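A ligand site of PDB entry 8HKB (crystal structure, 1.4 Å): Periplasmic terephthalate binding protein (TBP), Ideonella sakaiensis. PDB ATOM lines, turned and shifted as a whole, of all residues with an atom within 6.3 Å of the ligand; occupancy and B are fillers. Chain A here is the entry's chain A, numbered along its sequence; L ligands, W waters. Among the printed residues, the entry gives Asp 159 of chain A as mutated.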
ATOM      1  N   TYR A  12     -16.469 -19.939  10.567  1.00  0.00           N
ATOM      2  CA  TYR A  12     -16.427 -19.207  11.825  1.00  0.00           C
ATOM      3  C   TYR A  12     -15.951 -20.169  12.913  1.00  0.00           C
ATOM      4  O   TYR A  12     -16.093 -21.381  12.788  1.00  0.00           O
ATOM      5  CB  TYR A  12     -17.818 -18.640  12.206  1.00  0.00           C
ATOM      6  CG  TYR A  12     -18.279 -17.627  11.176  1.00  0.00           C
ATOM      7  CD1 TYR A  12     -17.831 -16.339  11.203  1.00  0.00           C
ATOM      8  CD2 TYR A  12     -19.145 -18.007  10.181  1.00  0.00           C
ATOM      9  CE1 TYR A  12     -18.180 -15.420  10.220  1.00  0.00           C
ATOM     10  CE2 TYR A  12     -19.496 -17.115   9.173  1.00  0.00           C
ATOM     11  CZ  TYR A  12     -19.057 -15.820   9.222  1.00  0.00           C
ATOM     12  OH  TYR A  12     -19.407 -14.921   8.236  1.00  0.00           O
ATOM     13  N   PRO A  13     -15.306 -19.610  13.977  1.00  0.00           N
ATOM     14  CA  PRO A  13     -14.847 -20.448  15.058  1.00  0.00           C
ATOM     15  C   PRO A  13     -15.968 -21.177  15.758  1.00  0.00           C
ATOM     16  O   PRO A  13     -17.121 -20.716  15.880  1.00  0.00           O
ATOM     17  CB  PRO A  13     -14.175 -19.474  16.071  1.00  0.00           C
ATOM     18  CG  PRO A  13     -14.370 -18.087  15.508  1.00  0.00           C
ATOM     19  CD  PRO A  13     -15.042 -18.193  14.181  1.00  0.00           C
ATOM     20  N   GLY A  15     -18.223 -22.633  18.759  1.00  0.00           N
ATOM     21  CA  GLY A  15     -18.730 -21.977  19.940  1.00  0.00           C
ATOM     22  C   GLY A  15     -19.994 -21.185  19.650  1.00  0.00           C
ATOM     23  O   GLY A  15     -20.908 -21.199  20.454  1.00  0.00           O
ATOM     24  N   GLY A  16     -20.033 -20.530  18.476  1.00  0.00           N
ATOM     25  CA  GLY A  16     -21.179 -19.694  18.145  1.00  0.00           C
ATOM     26  C   GLY A  16     -22.265 -20.472  17.439  1.00  0.00           C
ATOM     27  O   GLY A  16     -22.217 -21.668  17.294  1.00  0.00           O
ATOM     28  N   THR A  17     -23.303 -19.762  16.986  1.00  0.00           N
ATOM     29  CA  THR A  17     -24.448 -20.403  16.381  1.00  0.00           C
ATOM     30  C   THR A  17     -24.084 -20.977  15.001  1.00  0.00           C
ATOM     31  O   THR A  17     -24.621 -22.006  14.619  1.00  0.00           O
ATOM     32  CB  THR A  17     -25.612 -19.405  16.283  1.00  0.00           C
ATOM     33  OG1 THR A  17     -25.811 -18.846  17.598  1.00  0.00           O
ATOM     34  CG2 THR A  17     -26.871 -20.025  15.761  1.00  0.00           C
ATOM     35  N   ALA A  18     -23.208 -20.301  14.256  1.00  0.00           N
ATOM     36  CA  ALA A  18     -22.806 -20.830  12.953  1.00  0.00           C
ATOM     37  C   ALA A  18     -22.266 -22.270  13.045  1.00  0.00           C
ATOM     38  O   ALA A  18     -22.533 -23.081  12.175  1.00  0.00           O
ATOM     39  CB  ALA A  18     -21.789 -19.919  12.282  1.00  0.00           C
ATOM     40  N   ASP A  19     -21.503 -22.537  14.105  1.00  0.00           N
ATOM     41  CA  ASP A  19     -20.927 -23.855  14.360  1.00  0.00           C
ATOM     42  C   ASP A  19     -21.962 -24.812  14.952  1.00  0.00           C
ATOM     43  O   ASP A  19     -22.066 -25.958  14.500  1.00  0.00           O
ATOM     44  CB  ASP A  19     -19.712 -23.687  15.273  1.00  0.00           C
ATOM     45  CG  ASP A  19     -19.104 -25.006  15.698  1.00  0.00           C
ATOM     46  OD1 ASP A  19     -18.388 -25.644  14.893  1.00  0.00           O
ATOM     47  OD2 ASP A  19     -19.421 -25.374  16.825  1.00  0.00           O
ATOM     48  N   PRO A  68     -23.766 -18.384   8.050  1.00  0.00           N
ATOM     49  CA  PRO A  68     -24.582 -17.183   8.107  1.00  0.00           C
ATOM     50  C   PRO A  68     -24.355 -16.282   6.919  1.00  0.00           C
ATOM     51  O   PRO A  68     -23.579 -16.618   6.001  1.00  0.00           O
ATOM     52  CB  PRO A  68     -24.264 -16.583   9.476  1.00  0.00           C
ATOM     53  CG  PRO A  68     -22.872 -17.053   9.754  1.00  0.00           C
ATOM     54  CD  PRO A  68     -22.764 -18.422   9.135  1.00  0.00           C
ATOM     55  N   PRO A  69     -25.044 -15.150   6.823  1.00  0.00           N
ATOM     56  CA  PRO A  69     -25.172 -14.460   5.529  1.00  0.00           C
ATOM     57  C   PRO A  69     -23.965 -13.801   4.922  1.00  0.00           C
ATOM     58  O   PRO A  69     -24.018 -13.555   3.708  1.00  0.00           O
ATOM     59  CB  PRO A  69     -26.212 -13.391   5.864  1.00  0.00           C
ATOM     60  CG  PRO A  69     -27.041 -14.005   6.942  1.00  0.00           C
ATOM     61  CD  PRO A  69     -26.030 -14.669   7.832  1.00  0.00           C
ATOM     62  N   GLY A  70     -22.929 -13.473   5.653  1.00  0.00           N
ATOM     63  CA  GLY A  70     -21.854 -12.682   5.129  1.00  0.00           C
ATOM     64  C   GLY A  70     -21.323 -13.147   3.788  1.00  0.00           C
ATOM     65  O   GLY A  70     -21.417 -12.400   2.797  1.00  0.00           O
ATOM     66  N   ILE A  74     -24.069 -10.927   1.666  1.00  0.00           N
ATOM     67  CA  ILE A  74     -23.777  -9.570   2.143  1.00  0.00           C
ATOM     68  C   ILE A  74     -22.424  -9.032   1.667  1.00  0.00           C
ATOM     69  O   ILE A  74     -22.354  -7.913   1.129  1.00  0.00           O
ATOM     70  CB  ILE A  74     -23.892  -9.427   3.663  1.00  0.00           C
ATOM     71  CG1 ILE A  74     -25.264  -9.871   4.126  1.00  0.00           C
ATOM     72  CG2 ILE A  74     -23.602  -7.999   4.092  1.00  0.00           C
ATOM     73  CD1 ILE A  74     -25.489  -9.721   5.635  1.00  0.00           C
ATOM     74  N   ASN A 100     -31.467 -11.329  15.596  1.00  0.00           N
ATOM     75  CA  ASN A 100     -30.395 -10.626  16.269  1.00  0.00           C
ATOM     76  C   ASN A 100     -30.959  -9.848  17.455  1.00  0.00           C
ATOM     77  O   ASN A 100     -32.186  -9.590  17.596  1.00  0.00           O
ATOM     78  CB  ASN A 100     -29.587  -9.712  15.338  1.00  0.00           C
ATOM     79  CG  ASN A 100     -28.610 -10.413  14.422  1.00  0.00           C
ATOM     80  OD1 ASN A 100     -28.104  -9.771  13.433  1.00  0.00           O
ATOM     81  ND2 ASN A 100     -28.320 -11.634  14.714  1.00  0.00           N
ATOM     82  N   GLN A 132     -18.910 -10.069  14.445  1.00  0.00           N
ATOM     83  CA  GLN A 132     -18.477 -11.356  13.981  1.00  0.00           C
ATOM     84  C   GLN A 132     -17.560 -11.249  12.766  1.00  0.00           C
ATOM     85  O   GLN A 132     -17.146 -12.290  12.236  1.00  0.00           O
ATOM     86  CB  GLN A 132     -19.714 -12.165  13.545  1.00  0.00           C
ATOM     87  CG  GLN A 132     -20.730 -12.383  14.666  1.00  0.00           C
ATOM     88  CD  GLN A 132     -22.173 -12.249  14.230  1.00  0.00           C
ATOM     89  OE1 GLN A 132     -22.499 -11.585  13.241  1.00  0.00           O
ATOM     90  NE2 GLN A 132     -23.118 -12.733  15.054  1.00  0.00           N
ATOM     91  N   GLY A 135     -19.048  -7.409   7.273  1.00  0.00           N
ATOM     92  CA  GLY A 135     -20.146  -7.876   6.420  1.00  0.00           C
ATOM     93  C   GLY A 135     -21.019  -8.932   7.076  1.00  0.00           C
ATOM     94  O   GLY A 135     -21.931  -9.403   6.434  1.00  0.00           O
ATOM     95  N   THR A 136     -20.774  -9.274   8.332  1.00  0.00           N
ATOM     96  CA  THR A 136     -21.644 -10.167   9.098  1.00  0.00           C
ATOM     97  C   THR A 136     -22.868  -9.409   9.511  1.00  0.00           C
ATOM     98  O   THR A 136     -22.916  -8.176   9.501  1.00  0.00           O
ATOM     99  CB  THR A 136     -20.928 -10.766  10.316  1.00  0.00           C
ATOM    100  OG1 THR A 136     -20.604  -9.694  11.198  1.00  0.00           O
ATOM    101  CG2 THR A 136     -19.715 -11.567   9.916  1.00  0.00           C
ATOM    102  N   THR A 137     -23.934 -10.120   9.865  1.00  0.00           N
ATOM    103  CA  THR A 137     -25.151  -9.418  10.248  1.00  0.00           C
ATOM    104  C   THR A 137     -24.926  -8.569  11.494  1.00  0.00           C
ATOM    105  O   THR A 137     -25.548  -7.516  11.654  1.00  0.00           O
ATOM    106  CB  THR A 137     -26.425 -10.237  10.393  1.00  0.00           C
ATOM    107  OG1 THR A 137     -26.320 -11.068  11.571  1.00  0.00           O
ATOM    108  CG2 THR A 137     -26.710 -11.020   9.132  1.00  0.00           C
ATOM    109  N   SER A 138     -24.066  -9.001  12.426  1.00  0.00           N
ATOM    110  CA  SER A 138     -23.827  -8.149  13.590  1.00  0.00           C
ATOM    111  C   SER A 138     -23.215  -6.791  13.241  1.00  0.00           C
ATOM    112  O   SER A 138     -23.544  -5.778  13.852  1.00  0.00           O
ATOM    113  CB  SER A 138     -22.920  -8.834  14.566  1.00  0.00           C
ATOM    114  OG  SER A 138     -21.646  -9.153  14.014  1.00  0.00           O
ATOM    115  N   ASP A 159     -13.539 -12.519  14.572  1.00  0.00           N
ATOM    116  CA  ASP A 159     -13.654 -13.473  13.493  1.00  0.00           C
ATOM    117  C   ASP A 159     -14.899 -14.356  13.656  1.00  0.00           C
ATOM    118  O   ASP A 159     -15.162 -15.220  12.848  1.00  0.00           O
ATOM    119  CB  ASP A 159     -12.368 -14.277  13.271  1.00  0.00           C
ATOM    120  CG  ASP A 159     -11.125 -13.418  13.074  1.00  0.00           C
ATOM    121  OD1 ASP A 159     -11.184 -12.399  12.323  1.00  0.00           O
ATOM    122  OD2 ASP A 159     -10.092 -13.694  13.717  1.00  0.00           O
ATOM    123  N   GLY A 160     -15.677 -14.093  14.703  1.00  0.00           N
ATOM    124  CA  GLY A 160     -16.985 -14.724  14.885  1.00  0.00           C
ATOM    125  C   GLY A 160     -17.568 -14.380  16.239  1.00  0.00           C
ATOM    126  O   GLY A 160     -16.980 -13.611  16.988  1.00  0.00           O
ATOM    127  N   THR A 161     -18.754 -14.890  16.515  1.00  0.00           N
ATOM    128  CA  THR A 161     -19.397 -14.737  17.808  1.00  0.00           C
ATOM    129  C   THR A 161     -18.491 -15.169  18.962  1.00  0.00           C
ATOM    130  O   THR A 161     -18.478 -14.473  19.971  1.00  0.00           O
ATOM    131  CB  THR A 161     -20.729 -15.480  17.829  1.00  0.00           C
ATOM    132  OG1 THR A 161     -21.729 -14.770  17.078  1.00  0.00           O
ATOM    133  CG2 THR A 161     -21.244 -15.706  19.229  1.00  0.00           C
ATOM    134  N   ALA A 162     -17.858 -16.333  18.852  1.00  0.00           N
ATOM    135  CA  ALA A 162     -17.262 -16.905  20.063  1.00  0.00           C
ATOM    136  C   ALA A 162     -16.201 -15.963  20.647  1.00  0.00           C
ATOM    137  O   ALA A 162     -16.254 -15.653  21.846  1.00  0.00           O
ATOM    138  CB  ALA A 162     -16.701 -18.271  19.729  1.00  0.00           C
ATOM    139  N   PRO A 163     -15.210 -15.473  19.892  1.00  0.00           N
ATOM    140  CA  PRO A 163     -14.222 -14.531  20.440  1.00  0.00           C
ATOM    141  C   PRO A 163     -14.834 -13.196  20.905  1.00  0.00           C
ATOM    142  O   PRO A 163     -14.471 -12.591  21.945  1.00  0.00           O
ATOM    143  CB  PRO A 163     -13.206 -14.333  19.316  1.00  0.00           C
ATOM    144  CG  PRO A 163     -13.960 -14.736  18.085  1.00  0.00           C
ATOM    145  CD  PRO A 163     -14.871 -15.852  18.508  1.00  0.00           C
ATOM    146  N   ASP A 178     -25.272  -9.598  18.451  1.00  0.00           N
ATOM    147  CA  ASP A 178     -25.267 -11.018  18.207  1.00  0.00           C
ATOM    148  C   ASP A 178     -26.642 -11.551  17.850  1.00  0.00           C
ATOM    149  O   ASP A 178     -27.626 -10.889  18.006  1.00  0.00           O
ATOM    150  CB  ASP A 178     -24.791 -11.739  19.481  1.00  0.00           C
ATOM    151  CG  ASP A 178     -24.231 -13.129  19.285  1.00  0.00           C
ATOM    152  OD1 ASP A 178     -23.882 -13.526  18.172  1.00  0.00           O
ATOM    153  OD2 ASP A 178     -24.187 -13.898  20.295  1.00  0.00           O
ATOM    154  N   ASN A 179     -26.734 -12.845  17.483  1.00  0.00           N
ATOM    155  CA  ASN A 179     -28.008 -13.508  17.442  1.00  0.00           C
ATOM    156  C   ASN A 179     -28.381 -14.064  18.835  1.00  0.00           C
ATOM    157  O   ASN A 179     -27.549 -14.294  19.724  1.00  0.00           O
ATOM    158  CB  ASN A 179     -28.096 -14.585  16.360  1.00  0.00           C
ATOM    159  CG  ASN A 179     -27.041 -15.636  16.496  1.00  0.00           C
ATOM    160  OD1 ASN A 179     -25.940 -15.552  15.885  1.00  0.00           O
ATOM    161  ND2 ASN A 179     -27.307 -16.625  17.325  1.00  0.00           N
ATOM    162  N   SER A 182     -26.713 -17.680  20.588  1.00  0.00           N
ATOM    163  CA  SER A 182     -25.442 -17.746  21.252  1.00  0.00           C
ATOM    164  C   SER A 182     -25.426 -16.870  22.507  1.00  0.00           C
ATOM    165  O   SER A 182     -24.703 -17.208  23.456  1.00  0.00           O
ATOM    166  CB  SER A 182     -24.343 -17.464  20.269  1.00  0.00           C
ATOM    167  OG  SER A 182     -24.645 -16.343  19.452  1.00  0.00           O
ATOM    168  N   THR A 224     -31.136 -13.017  11.311  1.00  0.00           N
ATOM    169  CA  THR A 224     -30.085 -13.723  10.583  1.00  0.00           C
ATOM    170  C   THR A 224     -30.547 -15.145  10.279  1.00  0.00           C
ATOM    171  O   THR A 224     -31.691 -15.530  10.533  1.00  0.00           O
ATOM    172  CB  THR A 224     -28.754 -13.631  11.322  1.00  0.00           C
ATOM    173  OG1 THR A 224     -27.741 -14.044  10.384  1.00  0.00           O
ATOM    174  CG2 THR A 224     -28.709 -14.527  12.533  1.00  0.00           C
ATOM    175  N   TRP A 225     -29.651 -15.890   9.636  1.00  0.00           N
ATOM    176  CA  TRP A 225     -30.024 -17.197   9.122  1.00  0.00           C
ATOM    177  C   TRP A 225     -28.764 -17.964   8.807  1.00  0.00           C
ATOM    178  O   TRP A 225     -27.663 -17.379   8.703  1.00  0.00           O
ATOM    179  CB  TRP A 225     -30.927 -17.136   7.882  1.00  0.00           C
ATOM    180  CG  TRP A 225     -30.613 -16.086   6.867  1.00  0.00           C
ATOM    181  CD1 TRP A 225     -31.060 -14.809   6.872  1.00  0.00           C
ATOM    182  CD2 TRP A 225     -29.706 -16.199   5.746  1.00  0.00           C
ATOM    183  NE1 TRP A 225     -30.552 -14.148   5.774  1.00  0.00           N
ATOM    184  CE2 TRP A 225     -29.701 -14.954   5.082  1.00  0.00           C
ATOM    185  CE3 TRP A 225     -28.876 -17.202   5.254  1.00  0.00           C
ATOM    186  CZ2 TRP A 225     -28.980 -14.734   3.901  1.00  0.00           C
ATOM    187  CZ3 TRP A 225     -28.109 -16.966   4.144  1.00  0.00           C
ATOM    188  CH2 TRP A 225     -28.155 -15.739   3.481  1.00  0.00           C
ATOM    189  N   PHE A 226     -28.909 -19.264   8.666  1.00  0.00           N
ATOM    190  CA  PHE A 226     -27.779 -20.204   8.552  1.00  0.00           C
ATOM    191  C   PHE A 226     -28.120 -21.112   7.385  1.00  0.00           C
ATOM    192  O   PHE A 226     -29.098 -21.912   7.472  1.00  0.00           O
ATOM    193  CB  PHE A 226     -27.631 -20.950   9.874  1.00  0.00           C
ATOM    194  CG  PHE A 226     -27.274 -20.000  10.977  1.00  0.00           C
ATOM    195  CD1 PHE A 226     -28.275 -19.350  11.722  1.00  0.00           C
ATOM    196  CD2 PHE A 226     -25.953 -19.668  11.220  1.00  0.00           C
ATOM    197  CE1 PHE A 226     -27.941 -18.376  12.637  1.00  0.00           C
ATOM    198  CE2 PHE A 226     -25.647 -18.742  12.179  1.00  0.00           C
ATOM    199  CZ  PHE A 226     -26.621 -18.084  12.873  1.00  0.00           C
HETATM  200  C1  LIG L   1     -21.832 -14.551  11.931  1.00  0.00           C
HETATM  201  C2  LIG L   1     -21.053 -15.382  12.727  1.00  0.00           C
HETATM  202  C3  LIG L   1     -21.633 -16.268  13.616  1.00  0.00           C
HETATM  203  C4  LIG L   1     -23.034 -16.304  13.676  1.00  0.00           C
HETATM  204  C5  LIG L   1     -23.791 -15.457  12.902  1.00  0.00           C
HETATM  205  C6  LIG L   1     -23.208 -14.536  12.039  1.00  0.00           C
HETATM  206  C7  LIG L   1     -24.042 -13.586  11.279  1.00  0.00           C
HETATM  207  C8  LIG L   1     -20.801 -17.174  14.476  1.00  0.00           C
HETATM  208  O1  LIG L   1     -23.555 -12.936  10.303  1.00  0.00           O
HETATM  209  O2  LIG L   1     -25.267 -13.454  11.611  1.00  0.00           O
HETATM  210  O3  LIG L   1     -21.358 -18.164  15.030  1.00  0.00           O
HETATM  211  O4  LIG L   1     -19.607 -16.842  14.636  1.00  0.00           O
HETATM  212  O   HOH W   1     -25.893 -13.031  14.255  1.00  0.00           O
HETATM  213  O   HOH W   2     -23.628 -16.893  16.982  1.00  0.00           O
HETATM  214  O   HOH W   3     -22.118 -13.975   8.266  1.00  0.00           O
HETATM  215  O   HOH W   4     -19.889 -20.447  15.376  1.00  0.00           O
HETATM  216  O   HOH W   5     -17.966 -17.954  16.483  1.00  0.00           O
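Water W3 lies within hydrogen-bond range of O1 of the ligand (2.7 Å), N of Gly 70 (2.8 Å) and OH of Tyr 12 (2.9 Å).
Water W5 lies within hydrogen-bond range of O4 of the ligand (2.7 Å), N of Ala 162 (2.9 Å), O of Pro 13 (3.0 Å) and N of Thr 161 (3.2 Å).
Water W4 lies within hydrogen-bond range of an oxygen (O3) of the ligand (2.7 Å), the backbone carbonyl oxygen of Pro 13 (2.8 Å), the backbone NH of Asp 19 (2.9 Å) and the backbone NH of Gly 16 (3.1 Å).
Water W1 lies within hydrogen-bond range of an oxygen (O2) of the ligand (2.7 Å), the side-chain amide nitrogen (ND2) of Asn 100 (2.8 Å), the side-chain amide nitrogen (NE2) of Gln 132 (2.9 Å), the side-chain amide oxygen (OD1) of Asn 179 (3.0 Å) and the side-chain hydroxyl (OG1) of Thr 137 (3.4 Å).
Water W2 lies within hydrogen-bond range of OG of Ser 182 (2.7 Å), OG1 of Thr 161 (2.9 Å), N of Thr 17 (2.9 Å), OD1 of Asn 179 (2.9 Å) and O3 of the ligand (3.3 Å).
OD1 of Asn 100 sits at hydrogen-bond distance from OG1 of Thr 137.
The side-chain amide nitrogen (NE2) of Gln 132 lies within hydrogen-bond range of the side-chain hydroxyl (OG1) of Thr 161, at 3.2 Å.
The side-chain hydroxyl (OG1) of Thr 161 is in hydrogen-bond range of the side-chain carboxylate (OD1) of Asp 178 (2.7 Å).
The side-chain hydroxyl (OG1) of Thr 17 sits at hydrogen-bond distance from the side-chain hydroxyl (OG) of Ser 182 (3.3 Å).
The side-chain amide nitrogen (NE2) of Gln 132 lies within hydrogen-bond range of the side-chain carboxylate (OD1) of Asp 178 (3.3 Å).
The side-chain hydroxyl of Ser 138 is in hydrogen-bond range of the side-chain hydroxyl of Thr 136, at 3.1 Å.
The backbone NH (N) of Asn 179 lies close to the side-chain amide nitrogen (ND2) of Asn 100 (3.4 Å).
The backbone NH of Ile 74 lies within hydrogen-bond range of the backbone carbonyl oxygen of Pro 69.
Tyr 12 touches the ligand.
Gly 16 touches the ligand.
Pro 68 touches the ligand.
CD of Pro 69 touches O1 of the ligand (3.9 Å).
CB of Thr 136 touches O1 of the ligand, 3.4 Å away.
Gly 160 touches the ligand.
Asn 179 touches the ligand.
CE2 of Phe 226 touches C5 of the ligand, at 3.8 Å.
Hydrophobic or aromatic side chains within 4 Å of the ligand: Tyr 12, Ala 18, Pro 68, Pro 69 and Phe 226.
Of the 28 residues printed, 14 come within 4 Å of the ligand.
The nearest printed residue that does not touch the ligand is Asp 19 (4.5 Å).
The backbone NH (N) of Thr 137 is in hydrogen-bond range of an oxygen (O1) of the ligand, at 2.9 Å.
OG1 of Thr 137 is in hydrogen-bond range of O2 of the ligand (2.6 Å).
OG1 of Thr 224 is in hydrogen-bond range of O2 of the ligand (2.8 Å).
The backbone NH (N) of Thr 161 is in hydrogen-bond range of an oxygen (O4) of the ligand, 2.8 Å away.
The backbone NH (N) of Ala 18 lies within hydrogen-bond range of an oxygen (O3) of the ligand, 2.9 Å away.
The backbone NH (N) of Thr 17 sits at hydrogen-bond distance from an oxygen (O3) of the ligand, at 3.2 Å.
OE1 of Gln 132 lies close to O1 of the ligand, at 3.4 Å.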
